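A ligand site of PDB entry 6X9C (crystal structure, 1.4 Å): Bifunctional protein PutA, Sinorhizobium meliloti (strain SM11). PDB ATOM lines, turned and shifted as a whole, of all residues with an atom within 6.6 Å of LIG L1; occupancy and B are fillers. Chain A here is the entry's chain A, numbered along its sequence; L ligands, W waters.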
ATOM      1  N   GLU A 676      18.905   6.967   9.747  1.00  0.00           N
ATOM      2  CA  GLU A 676      19.036   7.895  10.864  1.00  0.00           C
ATOM      3  C   GLU A 676      17.713   8.029  11.603  1.00  0.00           C
ATOM      4  O   GLU A 676      17.682   8.091  12.835  1.00  0.00           O
ATOM      5  CB  GLU A 676      19.510   9.251  10.343  1.00  0.00           C
ATOM      6  CG  GLU A 676      19.936  10.223  11.447  1.00  0.00           C
ATOM      7  CD  GLU A 676      20.833  11.351  10.944  1.00  0.00           C
ATOM      8  OE1 GLU A 676      21.230  11.312   9.757  1.00  0.00           O
ATOM      9  OE2 GLU A 676      21.128  12.270  11.733  1.00  0.00           O
ATOM     10  N   PHE A 680      17.225   7.138  15.499  1.00  0.00           N
ATOM     11  CA  PHE A 680      16.647   8.029  16.502  1.00  0.00           C
ATOM     12  C   PHE A 680      15.552   7.323  17.304  1.00  0.00           C
ATOM     13  O   PHE A 680      15.530   7.386  18.531  1.00  0.00           O
ATOM     14  CB  PHE A 680      16.045   9.282  15.854  1.00  0.00           C
ATOM     15  CG  PHE A 680      17.028  10.392  15.577  1.00  0.00           C
ATOM     16  CD1 PHE A 680      17.915  10.846  16.551  1.00  0.00           C
ATOM     17  CD2 PHE A 680      17.047  11.011  14.335  1.00  0.00           C
ATOM     18  CE1 PHE A 680      18.785  11.878  16.285  1.00  0.00           C
ATOM     19  CE2 PHE A 680      17.921  12.047  14.052  1.00  0.00           C
ATOM     20  CZ  PHE A 680      18.809  12.487  15.024  1.00  0.00           C
ATOM     21  N   ASN A 709      15.887  19.886   4.849  1.00  0.00           N
ATOM     22  CA  ASN A 709      17.101  19.220   4.400  1.00  0.00           C
ATOM     23  C   ASN A 709      17.270  17.822   4.969  1.00  0.00           C
ATOM     24  O   ASN A 709      17.938  16.995   4.348  1.00  0.00           O
ATOM     25  CB  ASN A 709      18.330  20.087   4.688  1.00  0.00           C
ATOM     26  CG  ASN A 709      18.537  20.339   6.157  1.00  0.00           C
ATOM     27  OD1 ASN A 709      17.601  20.291   6.955  1.00  0.00           O
ATOM     28  ND2 ASN A 709      19.778  20.632   6.532  1.00  0.00           N
ATOM     29  N   PHE A 710      16.676  17.546   6.119  1.00  0.00           N
ATOM     30  CA  PHE A 710      16.551  16.187   6.632  1.00  0.00           C
ATOM     31  C   PHE A 710      15.094  15.988   7.003  1.00  0.00           C
ATOM     32  O   PHE A 710      14.722  15.950   8.187  1.00  0.00           O
ATOM     33  CB  PHE A 710      17.535  15.883   7.760  1.00  0.00           C
ATOM     34  CG  PHE A 710      18.911  15.592   7.265  1.00  0.00           C
ATOM     35  CD1 PHE A 710      19.781  16.618   6.966  1.00  0.00           C
ATOM     36  CD2 PHE A 710      19.305  14.294   7.013  1.00  0.00           C
ATOM     37  CE1 PHE A 710      21.039  16.363   6.492  1.00  0.00           C
ATOM     38  CE2 PHE A 710      20.562  14.020   6.527  1.00  0.00           C
ATOM     39  CZ  PHE A 710      21.435  15.058   6.269  1.00  0.00           C
ATOM     40  N   ILE A 714      15.485  14.412  10.983  1.00  0.00           N
ATOM     41  CA  ILE A 714      15.407  15.406  12.049  1.00  0.00           C
ATOM     42  C   ILE A 714      13.956  15.602  12.480  1.00  0.00           C
ATOM     43  O   ILE A 714      13.665  15.789  13.672  1.00  0.00           O
ATOM     44  CB  ILE A 714      16.090  16.717  11.615  1.00  0.00           C
ATOM     45  CG1 ILE A 714      17.603  16.551  11.721  1.00  0.00           C
ATOM     46  CG2 ILE A 714      15.600  17.914  12.466  1.00  0.00           C
ATOM     47  CD1 ILE A 714      18.344  17.656  11.039  1.00  0.00           C
ATOM     48  N   GLU A 812      18.968  23.718  16.951  1.00  0.00           N
ATOM     49  CA  GLU A 812      20.201  23.512  16.198  1.00  0.00           C
ATOM     50  C   GLU A 812      20.140  24.399  14.967  1.00  0.00           C
ATOM     51  O   GLU A 812      19.153  24.347  14.226  1.00  0.00           O
ATOM     52  CB  GLU A 812      20.399  22.055  15.774  1.00  0.00           C
ATOM     53  CG  GLU A 812      21.739  21.840  15.011  1.00  0.00           C
ATOM     54  CD  GLU A 812      21.569  21.549  13.533  1.00  0.00           C
ATOM     55  OE1 GLU A 812      21.182  20.407  13.190  1.00  0.00           O
ATOM     56  OE2 GLU A 812      21.817  22.447  12.709  1.00  0.00           O
ATOM     57  N   ARG A 845      23.639  20.154   4.095  1.00  0.00           N
ATOM     58  CA  ARG A 845      23.725  19.634   5.450  1.00  0.00           C
ATOM     59  C   ARG A 845      24.215  20.749   6.348  1.00  0.00           C
ATOM     60  O   ARG A 845      25.098  21.524   5.970  1.00  0.00           O
ATOM     61  CB  ARG A 845      24.749  18.498   5.522  1.00  0.00           C
ATOM     62  CG  ARG A 845      24.389  17.238   4.765  1.00  0.00           C
ATOM     63  CD  ARG A 845      25.482  16.213   4.977  1.00  0.00           C
ATOM     64  NE  ARG A 845      25.243  15.026   4.173  1.00  0.00           N
ATOM     65  CZ  ARG A 845      24.805  13.877   4.663  1.00  0.00           C
ATOM     66  NH1 ARG A 845      24.548  13.759   5.983  1.00  0.00           N
ATOM     67  NH2 ARG A 845      24.615  12.834   3.857  1.00  0.00           N
ATOM     68  N   CYS A 846      23.657  20.819   7.558  1.00  0.00           N
ATOM     69  CA  CYS A 846      24.184  21.767   8.525  1.00  0.00           C
ATOM     70  C   CYS A 846      25.653  21.494   8.819  1.00  0.00           C
ATOM     71  O   CYS A 846      26.385  22.429   9.186  1.00  0.00           O
ATOM     72  CB  CYS A 846      23.383  21.699   9.825  1.00  0.00           C
ATOM     73  SG  CYS A 846      23.503  20.101  10.637  1.00  0.00           S
ATOM     74  N   SER A 847      26.094  20.252   8.627  1.00  0.00           N
ATOM     75  CA  SER A 847      27.432  19.773   8.939  1.00  0.00           C
ATOM     76  C   SER A 847      28.404  19.947   7.781  1.00  0.00           C
ATOM     77  O   SER A 847      29.584  19.583   7.919  1.00  0.00           O
ATOM     78  CB  SER A 847      27.352  18.280   9.232  1.00  0.00           C
ATOM     79  OG  SER A 847      26.623  17.627   8.178  1.00  0.00           O
ATOM     80  N   ALA A 848      27.926  20.447   6.637  1.00  0.00           N
ATOM     81  CA  ALA A 848      28.729  20.452   5.418  1.00  0.00           C
ATOM     82  C   ALA A 848      29.991  21.286   5.583  1.00  0.00           C
ATOM     83  O   ALA A 848      30.031  22.274   6.319  1.00  0.00           O
ATOM     84  CB  ALA A 848      27.886  21.014   4.270  1.00  0.00           C
ATOM     85  N   THR A 973      30.395  21.381  13.211  1.00  0.00           N
ATOM     86  CA  THR A 973      31.341  20.341  12.848  1.00  0.00           C
ATOM     87  C   THR A 973      32.706  20.944  12.519  1.00  0.00           C
ATOM     88  O   THR A 973      32.828  22.115  12.152  1.00  0.00           O
ATOM     89  CB  THR A 973      30.846  19.499  11.660  1.00  0.00           C
ATOM     90  OG1 THR A 973      30.684  20.323  10.501  1.00  0.00           O
ATOM     91  CG2 THR A 973      29.527  18.802  12.004  1.00  0.00           C
ATOM     92  N   TYR A 997      36.082  15.605  13.791  1.00  0.00           N
ATOM     93  CA  TYR A 997      36.323  14.463  12.921  1.00  0.00           C
ATOM     94  C   TYR A 997      37.787  14.481  12.511  1.00  0.00           C
ATOM     95  O   TYR A 997      38.263  15.499  12.001  1.00  0.00           O
ATOM     96  CB  TYR A 997      35.419  14.515  11.684  1.00  0.00           C
ATOM     97  CG  TYR A 997      33.932  14.454  12.017  1.00  0.00           C
ATOM     98  CD1 TYR A 997      33.313  13.221  12.241  1.00  0.00           C
ATOM     99  CD2 TYR A 997      33.158  15.604  12.104  1.00  0.00           C
ATOM    100  CE1 TYR A 997      31.947  13.143  12.540  1.00  0.00           C
ATOM    101  CE2 TYR A 997      31.800  15.541  12.403  1.00  0.00           C
ATOM    102  CZ  TYR A 997      31.211  14.305  12.620  1.00  0.00           C
ATOM    103  OH  TYR A 997      29.866  14.236  12.920  1.00  0.00           O
ATOM    104  N   ILE A1002      33.363  15.011   7.562  1.00  0.00           N
ATOM    105  CA  ILE A1002      32.731  15.707   8.692  1.00  0.00           C
ATOM    106  C   ILE A1002      31.213  15.592   8.659  1.00  0.00           C
ATOM    107  O   ILE A1002      30.523  16.330   9.375  1.00  0.00           O
ATOM    108  CB  ILE A1002      33.211  17.159   8.842  1.00  0.00           C
ATOM    109  CG1 ILE A1002      32.668  18.068   7.730  1.00  0.00           C
ATOM    110  CG2 ILE A1002      34.721  17.182   8.893  1.00  0.00           C
ATOM    111  CD1 ILE A1002      33.021  19.528   7.922  1.00  0.00           C
ATOM    112  N   ILE A1003      30.658  14.663   7.874  1.00  0.00           N
ATOM    113  CA  ILE A1003      29.221  14.573   7.675  1.00  0.00           C
ATOM    114  C   ILE A1003      28.708  13.209   8.125  1.00  0.00           C
ATOM    115  O   ILE A1003      29.468  12.264   8.337  1.00  0.00           O
ATOM    116  CB  ILE A1003      28.784  14.873   6.221  1.00  0.00           C
ATOM    117  CG1 ILE A1003      29.384  13.855   5.239  1.00  0.00           C
ATOM    118  CG2 ILE A1003      29.136  16.289   5.831  1.00  0.00           C
ATOM    119  CD1 ILE A1003      28.675  13.849   3.863  1.00  0.00           C
ATOM    120  N   GLY A1004      27.382  13.117   8.222  1.00  0.00           N
ATOM    121  CA  GLY A1004      26.756  11.830   8.486  1.00  0.00           C
ATOM    122  C   GLY A1004      26.959  11.330   9.895  1.00  0.00           C
ATOM    123  O   GLY A1004      27.242  10.148  10.093  1.00  0.00           O
ATOM    124  N   ALA A1005      26.831  12.212  10.891  1.00  0.00           N
ATOM    125  CA  ALA A1005      26.911  11.781  12.274  1.00  0.00           C
ATOM    126  C   ALA A1005      25.909  10.659  12.527  1.00  0.00           C
ATOM    127  O   ALA A1005      24.781  10.694  12.016  1.00  0.00           O
ATOM    128  CB  ALA A1005      26.625  12.955  13.210  1.00  0.00           C
ATOM    129  N   VAL A1006      26.337   9.661  13.295  1.00  0.00           N
ATOM    130  CA  VAL A1006      25.574   8.452  13.580  1.00  0.00           C
ATOM    131  C   VAL A1006      24.991   8.593  14.973  1.00  0.00           C
ATOM    132  O   VAL A1006      25.714   8.864  15.946  1.00  0.00           O
ATOM    133  CB  VAL A1006      26.469   7.208  13.476  1.00  0.00           C
ATOM    134  CG1 VAL A1006      25.727   5.973  13.936  1.00  0.00           C
ATOM    135  CG2 VAL A1006      26.984   7.035  12.037  1.00  0.00           C
ATOM    136  N   PHE A1012      25.076  14.516  18.075  1.00  0.00           N
ATOM    137  CA  PHE A1012      25.265  15.609  17.142  1.00  0.00           C
ATOM    138  C   PHE A1012      24.712  16.920  17.681  1.00  0.00           C
ATOM    139  O   PHE A1012      23.550  16.994  18.092  1.00  0.00           O
ATOM    140  CB  PHE A1012      24.601  15.322  15.800  1.00  0.00           C
ATOM    141  CG  PHE A1012      24.865  16.380  14.796  1.00  0.00           C
ATOM    142  CD1 PHE A1012      26.073  16.384  14.104  1.00  0.00           C
ATOM    143  CD2 PHE A1012      23.959  17.393  14.552  1.00  0.00           C
ATOM    144  CE1 PHE A1012      26.365  17.386  13.194  1.00  0.00           C
ATOM    145  CE2 PHE A1012      24.239  18.401  13.641  1.00  0.00           C
ATOM    146  CZ  PHE A1012      25.447  18.391  12.946  1.00  0.00           C
HETATM  147  N1  LIG L   1      23.141  14.619  11.087  1.00  0.00           N
HETATM  148  C1  LIG L   1      23.492  15.026   9.726  1.00  0.00           C
HETATM  149  C2  LIG L   1      25.003  15.026   9.503  1.00  0.00           C
HETATM  150  O1  LIG L   1      25.448  15.184   8.366  1.00  0.00           O
HETATM  151  C3  LIG L   1      22.965  16.466   9.640  1.00  0.00           C
HETATM  152  C4  LIG L   1      21.991  16.597  10.774  1.00  0.00           C
HETATM  153  C5  LIG L   1      22.521  15.719  11.843  1.00  0.00           C
HETATM  154  O2  LIG L   1      25.798  14.884  10.434  1.00  0.00           O
HETATM  155  P1  LG2 L   2      13.948  28.549   8.211  1.00  0.00           P
HETATM  156  O1  LG2 L   2      14.743  28.300   9.467  1.00  0.00           O
HETATM  157  O2  LG2 L   2      13.199  29.788   7.840  1.00  0.00           O
HETATM  158  O3  LG2 L   2      12.719  27.331   8.295  1.00  0.00           O
HETATM  159  C1  LG2 L   2      13.043  26.425   9.278  1.00  0.00           C
HETATM  160  C2  LG2 L   2      11.685  25.978   9.934  1.00  0.00           C
HETATM  161  O4  LG2 L   2      11.201  27.079  10.676  1.00  0.00           O
HETATM  162  C3  LG2 L   2      10.586  25.655   8.852  1.00  0.00           C
HETATM  163  O5  LG2 L   2       9.741  24.650   9.380  1.00  0.00           O
HETATM  164  C4  LG2 L   2       9.831  26.970   8.742  1.00  0.00           C
HETATM  165  O6  LG2 L   2       8.503  26.787   8.365  1.00  0.00           O
HETATM  166  C5  LG2 L   2       9.881  27.401  10.231  1.00  0.00           C
HETATM  167  N1  LG2 L   2       9.747  28.811  10.419  1.00  0.00           N
HETATM  168  C6  LG2 L   2      10.127  29.867   9.559  1.00  0.00           C
HETATM  169  N2  LG2 L   2       9.859  31.065  10.097  1.00  0.00           N
HETATM  170  C7  LG2 L   2       9.295  30.783  11.343  1.00  0.00           C
HETATM  171  C8  LG2 L   2       8.817  31.624  12.378  1.00  0.00           C
HETATM  172  N3  LG2 L   2       8.846  32.980  12.271  1.00  0.00           N
HETATM  173  N4  LG2 L   2       8.302  31.080  13.518  1.00  0.00           N
HETATM  174  C9  LG2 L   2       8.302  29.727  13.590  1.00  0.00           C
HETATM  175  N5  LG2 L   2       8.720  28.804  12.692  1.00  0.00           N
HETATM  176  C10 LG2 L   2       9.224  29.393  11.573  1.00  0.00           C
HETATM  177  O7  LG2 L   2      14.989  27.964   7.139  1.00  0.00           O
HETATM  178  P2  LG2 L   2      14.790  28.419   5.586  1.00  0.00           P
HETATM  179  O8  LG2 L   2      14.391  29.824   5.263  1.00  0.00           O
HETATM  180  O9  LG2 L   2      14.233  27.166   4.966  1.00  0.00           O
HETATM  181  O10 LG2 L   2      16.402  28.330   5.009  1.00  0.00           O
HETATM  182  C11 LG2 L   2      16.996  29.523   5.371  1.00  0.00           C
HETATM  183  C12 LG2 L   2      18.400  29.252   5.908  1.00  0.00           C
HETATM  184  O11 LG2 L   2      18.287  28.644   7.193  1.00  0.00           O
HETATM  185  C13 LG2 L   2      19.119  28.189   5.036  1.00  0.00           C
HETATM  186  O12 LG2 L   2      19.684  28.806   3.919  1.00  0.00           O
HETATM  187  C14 LG2 L   2      20.184  27.730   6.050  1.00  0.00           C
HETATM  188  O13 LG2 L   2      21.248  28.644   6.201  1.00  0.00           O
HETATM  189  C15 LG2 L   2      19.375  27.732   7.391  1.00  0.00           C
HETATM  190  N6  LG2 L   2      18.809  26.395   7.672  1.00  0.00           N
HETATM  191  C16 LG2 L   2      19.429  25.544   8.572  1.00  0.00           C
HETATM  192  C17 LG2 L   2      19.025  24.242   8.647  1.00  0.00           C
HETATM  193  C18 LG2 L   2      19.769  23.331   9.503  1.00  0.00           C
HETATM  194  O14 LG2 L   2      19.913  22.109   9.268  1.00  0.00           O
HETATM  195  N7  LG2 L   2      20.305  23.853  10.641  1.00  0.00           N
HETATM  196  C19 LG2 L   2      18.114  23.655   7.609  1.00  0.00           C
HETATM  197  C20 LG2 L   2      17.268  24.684   7.011  1.00  0.00           C
HETATM  198  C21 LG2 L   2      17.631  25.964   7.014  1.00  0.00           C
HETATM  199  O   HOH W   1      23.833  11.904   9.791  1.00  0.00           O
HETATM  200  O   HOH W   2      21.572  19.113   8.324  1.00  0.00           O
HETATM  201  O   HOH W   3      20.325  15.635  14.547  1.00  0.00           O
HETATM  202  O   HOH W   4      28.510  15.559  11.143  1.00  0.00           O
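O1 of LIG L1 lies within hydrogen-bond range of N of Gly 1004, at 2.8 Å.
OE2 of Glu 676 is in salt-bridge range of N1 of LIG L1, 3.2 Å away.
An oxygen (O2) of LIG L1 sits at hydrogen-bond distance from the backbone NH (N) of Ala 1005, at 2.9 Å.
OE2 of Glu 812 lies within hydrogen-bond range of N7 of LG2 L2, at 2.9 Å.
NH1 of Arg 845 is in salt-bridge range of O1 of LIG L1.
O1 of LIG L1 is in hydrogen-bond range of OG of Ser 847.
The side-chain amide nitrogen of Asn 709 sits at hydrogen-bond distance from an oxygen (O14) of LG2 L2 (3.1 Å).
The side-chain hydroxyl (OG1) of Thr 973 is in hydrogen-bond range of the backbone carbonyl oxygen (O) of Ser 847, 2.9 Å away.
SG of Cys 846 lies within hydrogen-bond range of OE1 of Glu 812 (3.5 Å).
Residues that only touch LIG L1: Phe 710, Ile 714, Cys 846, Ile 1003 and Phe 1012.
Hydrophobic or aromatic side chains within 4 Å of LIG L1: Phe 710, Ile 714, Ile 1003, Ala 1005 and Phe 1012.
Ten residues have an atom within 4 Å of LIG L1: Glu 676, Phe 710, Ile 714, Arg 845, Cys 846, Ser 847, Ile 1003, Gly 1004, Ala 1005 and Phe 1012.
Water W4 lies within hydrogen-bond range of OH of Tyr 997 (2.6 Å), O of Ile 1002 (2.8 Å) and O2 of LIG L1 (2.9 Å).
Water W1 lies within hydrogen-bond range of OE1 of Glu 676 (2.7 Å), O of Ala 1005 (2.7 Å) and N1 of LIG L1 (3.1 Å).
Water W2 bridges the backbone NH (N) of Cys 846 (2.8 Å) and the side-chain amide nitrogen (ND2) of Asn 709 (3.0 Å).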
